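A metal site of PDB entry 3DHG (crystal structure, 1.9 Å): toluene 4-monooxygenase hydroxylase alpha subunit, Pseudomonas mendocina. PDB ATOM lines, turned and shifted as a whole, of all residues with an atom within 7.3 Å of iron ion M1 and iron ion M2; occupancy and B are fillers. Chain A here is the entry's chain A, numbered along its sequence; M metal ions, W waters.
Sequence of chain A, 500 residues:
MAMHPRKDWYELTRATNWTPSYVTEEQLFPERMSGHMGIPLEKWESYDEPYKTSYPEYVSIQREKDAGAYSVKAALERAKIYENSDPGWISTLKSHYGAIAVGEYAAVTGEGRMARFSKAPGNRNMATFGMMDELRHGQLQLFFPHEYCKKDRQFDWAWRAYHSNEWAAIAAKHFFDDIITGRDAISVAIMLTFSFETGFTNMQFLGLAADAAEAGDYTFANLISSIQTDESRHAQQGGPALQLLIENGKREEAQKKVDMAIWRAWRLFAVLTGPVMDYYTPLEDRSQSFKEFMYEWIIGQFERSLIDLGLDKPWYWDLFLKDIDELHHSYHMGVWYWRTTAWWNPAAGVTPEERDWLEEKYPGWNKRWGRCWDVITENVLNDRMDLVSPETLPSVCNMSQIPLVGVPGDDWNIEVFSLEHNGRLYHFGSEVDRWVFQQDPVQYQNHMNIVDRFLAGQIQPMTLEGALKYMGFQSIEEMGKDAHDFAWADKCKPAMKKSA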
ATOM      1  N   ILE A 100       6.699  -4.185  -2.575  1.00  0.00           N
ATOM      2  CA  ILE A 100       6.262  -3.298  -3.655  1.00  0.00           C
ATOM      3  C   ILE A 100       4.808  -2.824  -3.661  1.00  0.00           C
ATOM      4  O   ILE A 100       4.570  -1.638  -3.921  1.00  0.00           O
ATOM      5  CB  ILE A 100       6.709  -3.834  -5.065  1.00  0.00           C
ATOM      6  CG1 ILE A 100       8.246  -3.836  -5.188  1.00  0.00           C
ATOM      7  CG2 ILE A 100       6.007  -3.064  -6.221  1.00  0.00           C
ATOM      8  CD1 ILE A 100       8.944  -2.450  -5.034  1.00  0.00           C
ATOM      9  N   GLY A 103       3.640   0.051  -1.529  1.00  0.00           N
ATOM     10  CA  GLY A 103       4.562   1.131  -1.927  1.00  0.00           C
ATOM     11  C   GLY A 103       4.092   1.829  -3.204  1.00  0.00           C
ATOM     12  O   GLY A 103       4.260   3.055  -3.340  1.00  0.00           O
ATOM     13  N   GLU A 104       3.528   1.072  -4.135  1.00  0.00           N
ATOM     14  CA  GLU A 104       3.007   1.651  -5.400  1.00  0.00           C
ATOM     15  C   GLU A 104       1.828   2.529  -5.034  1.00  0.00           C
ATOM     16  O   GLU A 104       1.680   3.643  -5.559  1.00  0.00           O
ATOM     17  CB  GLU A 104       2.503   0.570  -6.348  1.00  0.00           C
ATOM     18  CG  GLU A 104       3.553  -0.383  -6.840  1.00  0.00           C
ATOM     19  CD  GLU A 104       4.046  -0.070  -8.229  1.00  0.00           C
ATOM     20  OE1 GLU A 104       3.872   1.084  -8.723  1.00  0.00           O
ATOM     21  OE2 GLU A 104       4.629  -1.007  -8.852  1.00  0.00           O
ATOM     22  N   TYR A 105       0.996   2.038  -4.124  1.00  0.00           N
ATOM     23  CA  TYR A 105      -0.116   2.852  -3.615  1.00  0.00           C
ATOM     24  C   TYR A 105       0.373   4.143  -2.910  1.00  0.00           C
ATOM     25  O   TYR A 105      -0.202   5.207  -3.126  1.00  0.00           O
ATOM     26  CB  TYR A 105      -1.077   2.030  -2.723  1.00  0.00           C
ATOM     27  CG  TYR A 105      -2.326   2.823  -2.445  1.00  0.00           C
ATOM     28  CD1 TYR A 105      -3.287   3.006  -3.449  1.00  0.00           C
ATOM     29  CD2 TYR A 105      -2.486   3.501  -1.241  1.00  0.00           C
ATOM     30  CE1 TYR A 105      -4.411   3.790  -3.202  1.00  0.00           C
ATOM     31  CE2 TYR A 105      -3.611   4.288  -0.984  1.00  0.00           C
ATOM     32  CZ  TYR A 105      -4.563   4.428  -1.937  1.00  0.00           C
ATOM     33  OH  TYR A 105      -5.655   5.224  -1.639  1.00  0.00           O
ATOM     34  N   ALA A 107       2.928   5.739  -3.786  1.00  0.00           N
ATOM     35  CA  ALA A 107       3.443   6.610  -4.875  1.00  0.00           C
ATOM     36  C   ALA A 107       2.328   7.525  -5.406  1.00  0.00           C
ATOM     37  O   ALA A 107       2.612   8.589  -5.929  1.00  0.00           O
ATOM     38  CB  ALA A 107       4.101   5.775  -5.998  1.00  0.00           C
ATOM     39  N   GLU A 111       2.798  11.483  -6.310  1.00  0.00           N
ATOM     40  CA  GLU A 111       2.195  12.046  -7.516  1.00  0.00           C
ATOM     41  C   GLU A 111       1.174  13.156  -7.159  1.00  0.00           C
ATOM     42  O   GLU A 111       1.204  14.232  -7.724  1.00  0.00           O
ATOM     43  CB  GLU A 111       1.576  10.949  -8.366  1.00  0.00           C
ATOM     44  CG  GLU A 111       2.653   9.990  -9.040  1.00  0.00           C
ATOM     45  CD  GLU A 111       3.496  10.658 -10.153  1.00  0.00           C
ATOM     46  OE1 GLU A 111       3.140  11.723 -10.651  1.00  0.00           O
ATOM     47  OE2 GLU A 111       4.557  10.111 -10.560  1.00  0.00           O
ATOM     48  N   GLY A 130      -0.003  10.280 -13.303  1.00  0.00           N
ATOM     49  CA  GLY A 130       0.824   9.459 -12.383  1.00  0.00           C
ATOM     50  C   GLY A 130       0.026   8.930 -11.194  1.00  0.00           C
ATOM     51  O   GLY A 130       0.238   7.750 -10.753  1.00  0.00           O
ATOM     52  N   ASP A 133      -1.853   6.015 -12.627  1.00  0.00           N
ATOM     53  CA  ASP A 133      -0.932   4.918 -12.912  1.00  0.00           C
ATOM     54  C   ASP A 133      -0.562   4.226 -11.633  1.00  0.00           C
ATOM     55  O   ASP A 133      -0.584   3.009 -11.560  1.00  0.00           O
ATOM     56  CB  ASP A 133       0.381   5.408 -13.541  1.00  0.00           C
ATOM     57  CG  ASP A 133       0.199   5.899 -14.936  1.00  0.00           C
ATOM     58  OD1 ASP A 133      -0.858   5.568 -15.566  1.00  0.00           O
ATOM     59  OD2 ASP A 133       1.131   6.599 -15.382  1.00  0.00           O
ATOM     60  N   GLU A 134      -0.217   4.996 -10.597  1.00  0.00           N
ATOM     61  CA  GLU A 134       0.232   4.271  -9.367  1.00  0.00           C
ATOM     62  C   GLU A 134      -0.932   3.587  -8.643  1.00  0.00           C
ATOM     63  O   GLU A 134      -0.739   2.544  -8.018  1.00  0.00           O
ATOM     64  CB  GLU A 134       1.062   5.133  -8.450  1.00  0.00           C
ATOM     65  CG  GLU A 134       2.265   5.814  -9.149  1.00  0.00           C
ATOM     66  CD  GLU A 134       3.387   4.885  -9.601  1.00  0.00           C
ATOM     67  OE1 GLU A 134       3.218   3.638  -9.676  1.00  0.00           O
ATOM     68  OE2 GLU A 134       4.439   5.472  -9.942  1.00  0.00           O
ATOM     69  N   LEU A 135      -2.113   4.065  -8.825  1.00  0.00           N
ATOM     70  CA  LEU A 135      -3.324   3.408  -8.336  1.00  0.00           C
ATOM     71  C   LEU A 135      -3.525   2.052  -9.006  1.00  0.00           C
ATOM     72  O   LEU A 135      -3.767   1.080  -8.387  1.00  0.00           O
ATOM     73  CB  LEU A 135      -4.551   4.292  -8.560  1.00  0.00           C
ATOM     74  CG  LEU A 135      -5.895   3.697  -8.147  1.00  0.00           C
ATOM     75  CD1 LEU A 135      -5.938   3.426  -6.652  1.00  0.00           C
ATOM     76  CD2 LEU A 135      -7.037   4.612  -8.566  1.00  0.00           C
ATOM     77  N   ARG A 136      -3.362   2.089 -10.337  1.00  0.00           N
ATOM     78  CA  ARG A 136      -3.416   0.843 -11.112  1.00  0.00           C
ATOM     79  C   ARG A 136      -2.430  -0.165 -10.550  1.00  0.00           C
ATOM     80  O   ARG A 136      -2.757  -1.340 -10.324  1.00  0.00           O
ATOM     81  CB  ARG A 136      -3.081   1.112 -12.585  1.00  0.00           C
ATOM     82  CG  ARG A 136      -3.126  -0.173 -13.433  1.00  0.00           C
ATOM     83  CD  ARG A 136      -2.675   0.069 -14.881  1.00  0.00           C
ATOM     84  NE  ARG A 136      -2.928  -1.162 -15.602  1.00  0.00           N
ATOM     85  CZ  ARG A 136      -2.045  -1.807 -16.370  1.00  0.00           C
ATOM     86  NH1 ARG A 136      -0.856  -1.286 -16.615  1.00  0.00           N
ATOM     87  NH2 ARG A 136      -2.391  -2.974 -16.938  1.00  0.00           N
ATOM     88  N   HIS A 137      -1.207   0.288 -10.304  1.00  0.00           N
ATOM     89  CA  HIS A 137      -0.134  -0.636  -9.929  1.00  0.00           C
ATOM     90  C   HIS A 137      -0.337  -1.239  -8.557  1.00  0.00           C
ATOM     91  O   HIS A 137      -0.127  -2.427  -8.371  1.00  0.00           O
ATOM     92  CB  HIS A 137       1.229   0.090 -10.041  1.00  0.00           C
ATOM     93  CG  HIS A 137       1.494   0.543 -11.437  1.00  0.00           C
ATOM     94  ND1 HIS A 137       2.536   1.397 -11.776  1.00  0.00           N
ATOM     95  CD2 HIS A 137       0.869   0.228 -12.604  1.00  0.00           C
ATOM     96  CE1 HIS A 137       2.498   1.612 -13.089  1.00  0.00           C
ATOM     97  NE2 HIS A 137       1.501   0.915 -13.613  1.00  0.00           N
ATOM     98  N   GLY A 138      -0.765  -0.404  -7.603  1.00  0.00           N
ATOM     99  CA  GLY A 138      -1.055  -0.865  -6.269  1.00  0.00           C
ATOM    100  C   GLY A 138      -2.228  -1.834  -6.294  1.00  0.00           C
ATOM    101  O   GLY A 138      -2.215  -2.836  -5.609  1.00  0.00           O
ATOM    102  N   GLN A 141      -1.190  -5.224  -8.014  1.00  0.00           N
ATOM    103  CA  GLN A 141      -0.245  -5.979  -7.192  1.00  0.00           C
ATOM    104  C   GLN A 141      -0.798  -6.369  -5.842  1.00  0.00           C
ATOM    105  O   GLN A 141      -0.070  -6.909  -5.012  1.00  0.00           O
ATOM    106  CB  GLN A 141       1.109  -5.254  -7.110  1.00  0.00           C
ATOM    107  CG  GLN A 141       1.738  -5.288  -8.515  1.00  0.00           C
ATOM    108  CD  GLN A 141       3.000  -4.521  -8.634  1.00  0.00           C
ATOM    109  OE1 GLN A 141       3.001  -3.295  -8.577  1.00  0.00           O
ATOM    110  NE2 GLN A 141       4.088  -5.241  -8.785  1.00  0.00           N
ATOM    111  N   LEU A 192      11.926  10.678  -6.769  1.00  0.00           N
ATOM    112  CA  LEU A 192      11.138   9.559  -7.175  1.00  0.00           C
ATOM    113  C   LEU A 192      11.208   9.354  -8.705  1.00  0.00           C
ATOM    114  O   LEU A 192      11.557   8.263  -9.157  1.00  0.00           O
ATOM    115  CB  LEU A 192       9.657   9.766  -6.723  1.00  0.00           C
ATOM    116  CG  LEU A 192       8.586   8.849  -7.317  1.00  0.00           C
ATOM    117  CD1 LEU A 192       8.836   7.373  -6.920  1.00  0.00           C
ATOM    118  CD2 LEU A 192       7.196   9.348  -6.892  1.00  0.00           C
ATOM    119  N   THR A 193      10.802  10.354  -9.491  1.00  0.00           N
ATOM    120  CA  THR A 193      10.558  10.072 -10.914  1.00  0.00           C
ATOM    121  C   THR A 193      11.866   9.963 -11.668  1.00  0.00           C
ATOM    122  O   THR A 193      12.018   9.019 -12.454  1.00  0.00           O
ATOM    123  CB  THR A 193       9.493  11.002 -11.609  1.00  0.00           C
ATOM    124  OG1 THR A 193      10.056  12.308 -11.867  1.00  0.00           O
ATOM    125  CG2 THR A 193       8.264  11.130 -10.762  1.00  0.00           C
ATOM    126  N   PHE A 196      14.654   7.294  -8.922  1.00  0.00           N
ATOM    127  CA  PHE A 196      14.202   5.930  -8.663  1.00  0.00           C
ATOM    128  C   PHE A 196      13.493   5.253  -9.848  1.00  0.00           C
ATOM    129  O   PHE A 196      13.860   4.178 -10.240  1.00  0.00           O
ATOM    130  CB  PHE A 196      13.314   5.865  -7.419  1.00  0.00           C
ATOM    131  CG  PHE A 196      12.925   4.461  -7.003  1.00  0.00           C
ATOM    132  CD1 PHE A 196      13.899   3.547  -6.565  1.00  0.00           C
ATOM    133  CD2 PHE A 196      11.598   4.063  -7.012  1.00  0.00           C
ATOM    134  CE1 PHE A 196      13.534   2.233  -6.157  1.00  0.00           C
ATOM    135  CE2 PHE A 196      11.213   2.762  -6.598  1.00  0.00           C
ATOM    136  CZ  PHE A 196      12.187   1.848  -6.160  1.00  0.00           C
ATOM    137  N   GLU A 197      12.450   5.883 -10.372  1.00  0.00           N
ATOM    138  CA  GLU A 197      11.651   5.297 -11.450  1.00  0.00           C
ATOM    139  C   GLU A 197      12.426   5.254 -12.760  1.00  0.00           C
ATOM    140  O   GLU A 197      12.600   4.191 -13.354  1.00  0.00           O
ATOM    141  CB  GLU A 197      10.311   6.031 -11.618  1.00  0.00           C
ATOM    142  CG  GLU A 197       9.354   5.844 -10.466  1.00  0.00           C
ATOM    143  CD  GLU A 197       8.084   6.678 -10.579  1.00  0.00           C
ATOM    144  OE1 GLU A 197       8.119   7.878 -10.935  1.00  0.00           O
ATOM    145  OE2 GLU A 197       7.035   6.115 -10.295  1.00  0.00           O
ATOM    146  N   THR A 201      13.601   1.429 -11.437  1.00  0.00           N
ATOM    147  CA  THR A 201      12.449   0.493 -11.529  1.00  0.00           C
ATOM    148  C   THR A 201      12.112   0.166 -12.970  1.00  0.00           C
ATOM    149  O   THR A 201      11.726  -0.947 -13.286  1.00  0.00           O
ATOM    150  CB  THR A 201      11.178   0.942 -10.766  1.00  0.00           C
ATOM    151  OG1 THR A 201      10.631   2.118 -11.375  1.00  0.00           O
ATOM    152  CG2 THR A 201      11.512   1.235  -9.349  1.00  0.00           C
ATOM    153  N   PHE A 205      11.908  -3.758 -13.677  1.00  0.00           N
ATOM    154  CA  PHE A 205      10.650  -4.429 -14.082  1.00  0.00           C
ATOM    155  C   PHE A 205      10.822  -5.157 -15.407  1.00  0.00           C
ATOM    156  O   PHE A 205      10.287  -6.249 -15.584  1.00  0.00           O
ATOM    157  CB  PHE A 205       9.498  -3.421 -14.133  1.00  0.00           C
ATOM    158  CG  PHE A 205       8.819  -3.231 -12.807  1.00  0.00           C
ATOM    159  CD1 PHE A 205       9.581  -3.120 -11.636  1.00  0.00           C
ATOM    160  CD2 PHE A 205       7.434  -3.190 -12.702  1.00  0.00           C
ATOM    161  CE1 PHE A 205       8.972  -2.952 -10.383  1.00  0.00           C
ATOM    162  CE2 PHE A 205       6.813  -3.039 -11.436  1.00  0.00           C
ATOM    163  CZ  PHE A 205       7.580  -2.918 -10.287  1.00  0.00           C
ATOM    164  N   ILE A 227       2.686  -3.319 -16.429  1.00  0.00           N
ATOM    165  CA  ILE A 227       2.921  -2.216 -15.496  1.00  0.00           C
ATOM    166  C   ILE A 227       4.075  -1.347 -15.974  1.00  0.00           C
ATOM    167  O   ILE A 227       3.992  -0.127 -15.953  1.00  0.00           O
ATOM    168  CB  ILE A 227       3.191  -2.783 -14.098  1.00  0.00           C
ATOM    169  CG1 ILE A 227       1.871  -3.250 -13.506  1.00  0.00           C
ATOM    170  CG2 ILE A 227       3.850  -1.738 -13.172  1.00  0.00           C
ATOM    171  CD1 ILE A 227       2.048  -4.062 -12.173  1.00  0.00           C
ATOM    172  N   ASP A 230       3.565   1.623 -18.333  1.00  0.00           N
ATOM    173  CA  ASP A 230       3.005   2.863 -17.755  1.00  0.00           C
ATOM    174  C   ASP A 230       4.058   3.844 -17.290  1.00  0.00           C
ATOM    175  O   ASP A 230       3.779   5.048 -17.146  1.00  0.00           O
ATOM    176  CB  ASP A 230       2.102   2.564 -16.553  1.00  0.00           C
ATOM    177  CG  ASP A 230       0.848   1.817 -16.931  1.00  0.00           C
ATOM    178  OD1 ASP A 230       0.376   1.957 -18.096  1.00  0.00           O
ATOM    179  OD2 ASP A 230       0.337   1.057 -16.081  1.00  0.00           O
ATOM    180  N   GLU A 231       5.251   3.321 -17.025  1.00  0.00           N
ATOM    181  CA  GLU A 231       6.276   4.036 -16.277  1.00  0.00           C
ATOM    182  C   GLU A 231       6.672   5.366 -16.933  1.00  0.00           C
ATOM    183  O   GLU A 231       6.603   6.403 -16.295  1.00  0.00           O
ATOM    184  CB  GLU A 231       7.516   3.152 -16.042  1.00  0.00           C
ATOM    185  CG  GLU A 231       8.375   3.608 -14.858  1.00  0.00           C
ATOM    186  CD  GLU A 231       7.610   3.454 -13.566  1.00  0.00           C
ATOM    187  OE1 GLU A 231       6.997   2.358 -13.378  1.00  0.00           O
ATOM    188  OE2 GLU A 231       7.555   4.401 -12.742  1.00  0.00           O
ATOM    189  N   SER A 232       7.061   5.326 -18.210  1.00  0.00           N
ATOM    190  CA  SER A 232       7.608   6.521 -18.876  1.00  0.00           C
ATOM    191  C   SER A 232       6.675   7.734 -18.823  1.00  0.00           C
ATOM    192  O   SER A 232       7.143   8.880 -18.735  1.00  0.00           O
ATOM    193  CB  SER A 232       8.002   6.203 -20.317  1.00  0.00           C
ATOM    194  OG  SER A 232       6.864   6.221 -21.154  1.00  0.00           O
ATOM    195  N   HIS A 234       4.824   8.941 -16.453  1.00  0.00           N
ATOM    196  CA  HIS A 234       4.990   9.780 -15.261  1.00  0.00           C
ATOM    197  C   HIS A 234       6.432   9.827 -14.776  1.00  0.00           C
ATOM    198  O   HIS A 234       6.844  10.779 -14.115  1.00  0.00           O
ATOM    199  CB  HIS A 234       4.081   9.321 -14.127  1.00  0.00           C
ATOM    200  CG  HIS A 234       4.311   7.913 -13.706  1.00  0.00           C
ATOM    201  ND1 HIS A 234       3.517   6.873 -14.129  1.00  0.00           N
ATOM    202  CD2 HIS A 234       5.241   7.358 -12.889  1.00  0.00           C
ATOM    203  CE1 HIS A 234       3.950   5.733 -13.598  1.00  0.00           C
ATOM    204  NE2 HIS A 234       4.987   6.001 -12.832  1.00  0.00           N
ATOM    205  N   ALA A 235       7.212   8.811 -15.089  1.00  0.00           N
ATOM    206  CA  ALA A 235       8.646   8.894 -14.726  1.00  0.00           C
ATOM    207  C   ALA A 235       9.391  10.061 -15.402  1.00  0.00           C
ATOM    208  O   ALA A 235      10.450  10.515 -14.922  1.00  0.00           O
ATOM    209  CB  ALA A 235       9.339   7.559 -15.026  1.00  0.00           C
HETATM  210 FE    FE M   1       5.952   4.724 -11.277  1.00  0.00          FE
HETATM  211 FE    FE M   2       4.254   2.085 -10.416  1.00  0.00          FE
HETATM  212  O   HOH W   1       5.069   3.115 -11.869  1.00  0.00           O
HETATM  213  O   HOH W   2       5.460   0.447 -10.941  1.00  0.00           O
HETATM  214  O   HOH W   3       6.454   3.371  -9.647  1.00  0.00           O
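OE1 of Gln 141 sits close to OE2 of Glu 104, at 2.8 Å. The backbone carbonyl oxygen (O) of Glu 197 sits close to the side-chain hydroxyl (OG1) of Thr 201 (3.5 Å). The backbone NH (N) of Glu 197 lies within hydrogen-bond range of the backbone carbonyl oxygen (O) of Leu 192 (2.8 Å). ND1 of His 234 sits at hydrogen-bond distance from OD2 of Asp 133 (2.7 Å). The backbone carbonyl oxygen (O) of His 137 sits close to the side-chain amide oxygen (OE1) of Gln 141. A ring nitrogen (NE2) of His 137 is in hydrogen-bond range of the side-chain carboxylate (OD2) of Asp 230, at 2.7 Å.
Of the 26 residues printed, 4 come within 4 Å of iron ion M1.
Three residues have an atom within 4 Å of iron ion M2: Glu 104, Glu 134 and His 137.
Water W1 binds iron ion M1 (1.9 Å). OE2 of Glu 197 binds iron ion M1. The side-chain carboxylate (OE2) of Glu 134 binds iron ion M1 (2.2 Å). Water W3 is bound to iron ion M1 (2.2 Å). Iron ion M1 is bound by OE2 of Glu 231 (2.2 Å). NE2 of His 234 is bound to iron ion M1.
Iron ion M2 is bound by water W1 (2.0 Å), the side-chain carboxylate of Glu 104 (2.0 Å), the side-chain carboxylate of Glu 134 (2.0 Å), water W2 (2.1 Å) and a ring nitrogen (ND1) of His 137 (2.3 Å). Slightly farther from iron ion M2 lies water W3 (2.7 Å).
Water W2 bridges the side-chain carboxylate of Glu 104 (2.7 Å) and the side-chain carboxylate of Glu 231 (3.5 Å).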
